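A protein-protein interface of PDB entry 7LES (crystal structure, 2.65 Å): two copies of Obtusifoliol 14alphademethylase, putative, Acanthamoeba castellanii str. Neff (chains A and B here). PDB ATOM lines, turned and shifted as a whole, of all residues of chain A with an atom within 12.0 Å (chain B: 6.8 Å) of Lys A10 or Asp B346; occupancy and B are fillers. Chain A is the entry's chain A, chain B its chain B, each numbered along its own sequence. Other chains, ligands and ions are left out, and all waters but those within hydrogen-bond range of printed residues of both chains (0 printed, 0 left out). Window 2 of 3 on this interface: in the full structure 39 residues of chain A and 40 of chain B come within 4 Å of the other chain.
Of the 7 printed residues of chain A, 6 touch a printed residue of chain B. Printed residues of chain A that touch a printed residue of chain B: Gly A9, Lys A10, Leu A11, Pro A12, Pro A13 and Val A14. Hydrophobic or aromatic side chains of chain A that line the printed part of chain B: Leu A11, Pro A12, Pro A13 and Val A14. Among the printed residues, 12 pairs touch across the chains.
The backbone carbonyl oxygen (O) of Lys A10 sits at hydrogen-bond distance from the backbone NH (N) of Tyr B348. OD1 of Asp B346 is in salt-bridge range of NZ of Lys A10, at 3.6 Å.
No position is printed for both chains.
Among the printed residues, pairs that only touch across the chains: Gly A9 with Tyr B348 (3.5 Å), Lys A10 with Tyr B347 (3.2 Å), Leu A11 with Arg B55 (3.9 Å), Leu A11 with Tyr B347 (3.98 Å), Leu A11 with Tyr B348 (3.97 Å), Pro A12 with Arg B55 (3.9 Å), Pro A12 with Tyr B347 (3.5 Å), Pro A12 with Tyr B348 (3.2 Å), Pro A13 with Tyr B347 (3.8 Å) and Val A14 with Arg B55 (3.5 Å).
Of the printed residues of chain B, Gly A9 touches Tyr B348 (3.5 Å). Of chain B, only Asp B346, Tyr B347 and Tyr B348 come within 4 Å of Lys A10. Of the printed residues of chain B, Val A14 touches Arg B55. Of the printed residues of chain A, Arg B55 touches Leu A11 (3.9 Å), Pro A12 (3.9 Å) and Val A14 (3.5 Å). No residue of chain A comes within 4 Å of Ser B343. No residue of chain A comes within 4 Å of Lys B345. Asp B346 touches just one residue of chain A: Lys A10. Printed residues of chain A within 4 Å of Tyr B348: Gly A9, Lys A10, Leu A11 and Pro A12. The nearest printed residue of chain A that does not touch Arg B55 is Pro A13 (6.4 Å).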
ATOM      1  N   LYS A   8      20.494   3.076 -21.220  1.00  0.00           N
ATOM      2  CA  LYS A   8      21.425   3.706 -22.201  1.00  0.00           C
ATOM      3  C   LYS A   8      21.900   2.672 -23.254  1.00  0.00           C
ATOM      4  O   LYS A   8      21.301   1.598 -23.419  1.00  0.00           O
ATOM      5  CB  LYS A   8      22.614   4.342 -21.452  1.00  0.00           C
ATOM      6  N   GLY A   9      22.950   3.031 -23.987  1.00  0.00           N
ATOM      7  CA  GLY A   9      23.688   2.100 -24.852  1.00  0.00           C
ATOM      8  C   GLY A   9      25.130   1.962 -24.375  1.00  0.00           C
ATOM      9  O   GLY A   9      25.516   2.574 -23.373  1.00  0.00           O
ATOM     10  N   LYS A  10      25.922   1.185 -25.117  1.00  0.00           N
ATOM     11  CA  LYS A  10      27.286   0.796 -24.712  1.00  0.00           C
ATOM     12  C   LYS A  10      28.309   1.952 -24.609  1.00  0.00           C
ATOM     13  O   LYS A  10      28.644   2.574 -25.615  1.00  0.00           O
ATOM     14  CB  LYS A  10      27.849  -0.265 -25.678  1.00  0.00           C
ATOM     15  CG  LYS A  10      27.151  -1.622 -25.645  1.00  0.00           C
ATOM     16  CD  LYS A  10      27.618  -2.538 -26.786  1.00  0.00           C
ATOM     17  CE  LYS A  10      26.953  -3.915 -26.756  1.00  0.00           C
ATOM     18  NZ  LYS A  10      26.699  -4.489 -28.111  1.00  0.00           N
ATOM     19  N   LEU A  11      28.834   2.211 -23.407  1.00  0.00           N
ATOM     20  CA  LEU A  11      29.922   3.172 -23.269  1.00  0.00           C
ATOM     21  C   LEU A  11      31.177   2.570 -23.882  1.00  0.00           C
ATOM     22  O   LEU A  11      31.493   1.396 -23.682  1.00  0.00           O
ATOM     23  CB  LEU A  11      30.192   3.567 -21.820  1.00  0.00           C
ATOM     24  CG  LEU A  11      29.017   4.093 -20.986  1.00  0.00           C
ATOM     25  CD1 LEU A  11      29.541   4.787 -19.728  1.00  0.00           C
ATOM     26  CD2 LEU A  11      28.108   5.020 -21.776  1.00  0.00           C
ATOM     27  N   PRO A  12      31.882   3.366 -24.673  1.00  0.00           N
ATOM     28  CA  PRO A  12      33.085   2.833 -25.282  1.00  0.00           C
ATOM     29  C   PRO A  12      34.234   2.643 -24.301  1.00  0.00           C
ATOM     30  O   PRO A  12      34.245   3.268 -23.225  1.00  0.00           O
ATOM     31  CB  PRO A  12      33.458   3.902 -26.320  1.00  0.00           C
ATOM     32  CG  PRO A  12      32.760   5.148 -25.885  1.00  0.00           C
ATOM     33  CD  PRO A  12      31.505   4.681 -25.229  1.00  0.00           C
ATOM     34  N   PRO A  13      35.219   1.826 -24.698  1.00  0.00           N
ATOM     35  CA  PRO A  13      36.359   1.483 -23.858  1.00  0.00           C
ATOM     36  C   PRO A  13      37.049   2.650 -23.147  1.00  0.00           C
ATOM     37  O   PRO A  13      37.766   3.420 -23.781  1.00  0.00           O
ATOM     38  CB  PRO A  13      37.339   0.784 -24.834  1.00  0.00           C
ATOM     39  CG  PRO A  13      36.669   0.706 -26.159  1.00  0.00           C
ATOM     40  CD  PRO A  13      35.231   1.079 -25.970  1.00  0.00           C
ATOM     41  N   VAL A  14      36.801   2.782 -21.843  1.00  0.00           N
ATOM     42  CA  VAL A  14      37.585   3.670 -20.961  1.00  0.00           C
ATOM     43  C   VAL A  14      38.937   3.024 -20.824  1.00  0.00           C
ATOM     44  O   VAL A  14      38.993   1.892 -20.400  1.00  0.00           O
ATOM     45  CB  VAL A  14      36.961   3.784 -19.559  1.00  0.00           C
ATOM     46  CG1 VAL A  14      37.904   4.513 -18.603  1.00  0.00           C
ATOM     47  CG2 VAL A  14      35.605   4.478 -19.637  1.00  0.00           C
ATOM     48  N   ARG B  55      34.906  12.780 -18.840  1.00  0.00           N
ATOM     49  CA  ARG B  55      35.110  11.764 -19.890  1.00  0.00           C
ATOM     50  C   ARG B  55      35.656  12.483 -21.150  1.00  0.00           C
ATOM     51  O   ARG B  55      35.075  13.477 -21.594  1.00  0.00           O
ATOM     52  CB  ARG B  55      33.793  10.966 -20.169  1.00  0.00           C
ATOM     53  CG  ARG B  55      33.285   9.979 -19.069  1.00  0.00           C
ATOM     54  CD  ARG B  55      31.943   9.285 -19.396  1.00  0.00           C
ATOM     55  NE  ARG B  55      31.929   8.740 -20.762  1.00  0.00           N
ATOM     56  CZ  ARG B  55      32.429   7.552 -21.141  1.00  0.00           C
ATOM     57  NH1 ARG B  55      32.947   6.693 -20.261  1.00  0.00           N
ATOM     58  NH2 ARG B  55      32.400   7.196 -22.425  1.00  0.00           N
ATOM     59  N   SER B 343      25.112   8.150 -31.221  1.00  0.00           N
ATOM     60  CA  SER B 343      25.508   6.758 -31.319  1.00  0.00           C
ATOM     61  C   SER B 343      26.577   6.670 -32.373  1.00  0.00           C
ATOM     62  O   SER B 343      26.618   7.490 -33.279  1.00  0.00           O
ATOM     63  CB  SER B 343      24.302   5.914 -31.686  1.00  0.00           C
ATOM     64  OG  SER B 343      23.201   6.292 -30.867  1.00  0.00           O
ATOM     65  N   TYR B 344      27.476   5.713 -32.219  1.00  0.00           N
ATOM     66  CA  TYR B 344      28.498   5.457 -33.221  1.00  0.00           C
ATOM     67  C   TYR B 344      28.804   3.978 -33.179  1.00  0.00           C
ATOM     68  O   TYR B 344      29.285   3.491 -32.166  1.00  0.00           O
ATOM     69  CB  TYR B 344      29.776   6.270 -32.985  1.00  0.00           C
ATOM     70  CG  TYR B 344      30.877   5.807 -33.919  1.00  0.00           C
ATOM     71  CD1 TYR B 344      30.702   5.870 -35.290  1.00  0.00           C
ATOM     72  CD2 TYR B 344      32.057   5.249 -33.441  1.00  0.00           C
ATOM     73  CE1 TYR B 344      31.673   5.415 -36.165  1.00  0.00           C
ATOM     74  CE2 TYR B 344      33.044   4.804 -34.313  1.00  0.00           C
ATOM     75  CZ  TYR B 344      32.836   4.892 -35.677  1.00  0.00           C
ATOM     76  OH  TYR B 344      33.767   4.446 -36.566  1.00  0.00           O
ATOM     77  N   LYS B 345      28.512   3.270 -34.269  1.00  0.00           N
ATOM     78  CA  LYS B 345      28.557   1.813 -34.284  1.00  0.00           C
ATOM     79  C   LYS B 345      27.702   1.265 -33.121  1.00  0.00           C
ATOM     80  O   LYS B 345      26.566   1.714 -32.941  1.00  0.00           O
ATOM     81  CB  LYS B 345      30.008   1.328 -34.223  1.00  0.00           C
ATOM     82  CG  LYS B 345      30.935   2.014 -35.209  1.00  0.00           C
ATOM     83  CD  LYS B 345      32.270   1.288 -35.309  1.00  0.00           C
ATOM     84  CE  LYS B 345      32.888   1.058 -33.932  1.00  0.00           C
ATOM     85  NZ  LYS B 345      34.349   0.804 -34.002  1.00  0.00           N
ATOM     86  N   ASP B 346      28.230   0.322 -32.333  1.00  0.00           N
ATOM     87  CA  ASP B 346      27.527  -0.139 -31.138  1.00  0.00           C
ATOM     88  C   ASP B 346      27.405   0.941 -30.087  1.00  0.00           C
ATOM     89  O   ASP B 346      26.418   0.973 -29.348  1.00  0.00           O
ATOM     90  CB  ASP B 346      28.250  -1.333 -30.520  1.00  0.00           C
ATOM     91  CG  ASP B 346      27.921  -2.623 -31.213  1.00  0.00           C
ATOM     92  OD1 ASP B 346      26.710  -2.928 -31.328  1.00  0.00           O
ATOM     93  OD2 ASP B 346      28.869  -3.329 -31.629  1.00  0.00           O
ATOM     94  N   TYR B 347      28.398   1.831 -30.030  1.00  0.00           N
ATOM     95  CA  TYR B 347      28.612   2.639 -28.831  1.00  0.00           C
ATOM     96  C   TYR B 347      27.651   3.815 -28.659  1.00  0.00           C
ATOM     97  O   TYR B 347      26.909   4.175 -29.576  1.00  0.00           O
ATOM     98  CB  TYR B 347      30.070   3.069 -28.730  1.00  0.00           C
ATOM     99  CG  TYR B 347      31.022   1.896 -28.747  1.00  0.00           C
ATOM    100  CD1 TYR B 347      31.144   1.055 -27.636  1.00  0.00           C
ATOM    101  CD2 TYR B 347      31.791   1.600 -29.886  1.00  0.00           C
ATOM    102  CE1 TYR B 347      32.021  -0.036 -27.649  1.00  0.00           C
ATOM    103  CE2 TYR B 347      32.672   0.513 -29.909  1.00  0.00           C
ATOM    104  CZ  TYR B 347      32.786  -0.297 -28.787  1.00  0.00           C
ATOM    105  OH  TYR B 347      33.650  -1.366 -28.798  1.00  0.00           O
ATOM    106  N   TYR B 348      27.632   4.335 -27.437  1.00  0.00           N
ATOM    107  CA  TYR B 348      26.812   5.465 -27.026  1.00  0.00           C
ATOM    108  C   TYR B 348      27.784   6.486 -26.420  1.00  0.00           C
ATOM    109  O   TYR B 348      28.682   6.101 -25.645  1.00  0.00           O
ATOM    110  CB  TYR B 348      25.793   5.021 -25.977  1.00  0.00           C
ATOM    111  CG  TYR B 348      24.845   6.113 -25.515  1.00  0.00           C
ATOM    112  CD1 TYR B 348      23.809   6.548 -26.341  1.00  0.00           C
ATOM    113  CD2 TYR B 348      24.967   6.699 -24.239  1.00  0.00           C
ATOM    114  CE1 TYR B 348      22.928   7.541 -25.931  1.00  0.00           C
ATOM    115  CE2 TYR B 348      24.088   7.693 -23.816  1.00  0.00           C
ATOM    116  CZ  TYR B 348      23.070   8.112 -24.670  1.00  0.00           C
ATOM    117  OH  TYR B 348      22.188   9.101 -24.300  1.00  0.00           O
ATOM    118  N   VAL B 349      27.624   7.761 -26.796  1.00  0.00           N
ATOM    119  CA  VAL B 349      28.462   8.839 -26.292  1.00  0.00           C
ATOM    120  C   VAL B 349      27.538   9.799 -25.537  1.00  0.00           C
ATOM    121  O   VAL B 349      26.718  10.461 -26.168  1.00  0.00           O
ATOM    122  CB  VAL B 349      29.259   9.542 -27.421  1.00  0.00           C
ATOM    123  CG1 VAL B 349      29.959  10.791 -26.905  1.00  0.00           C
ATOM    124  CG2 VAL B 349      30.309   8.604 -28.017  1.00  0.00           C
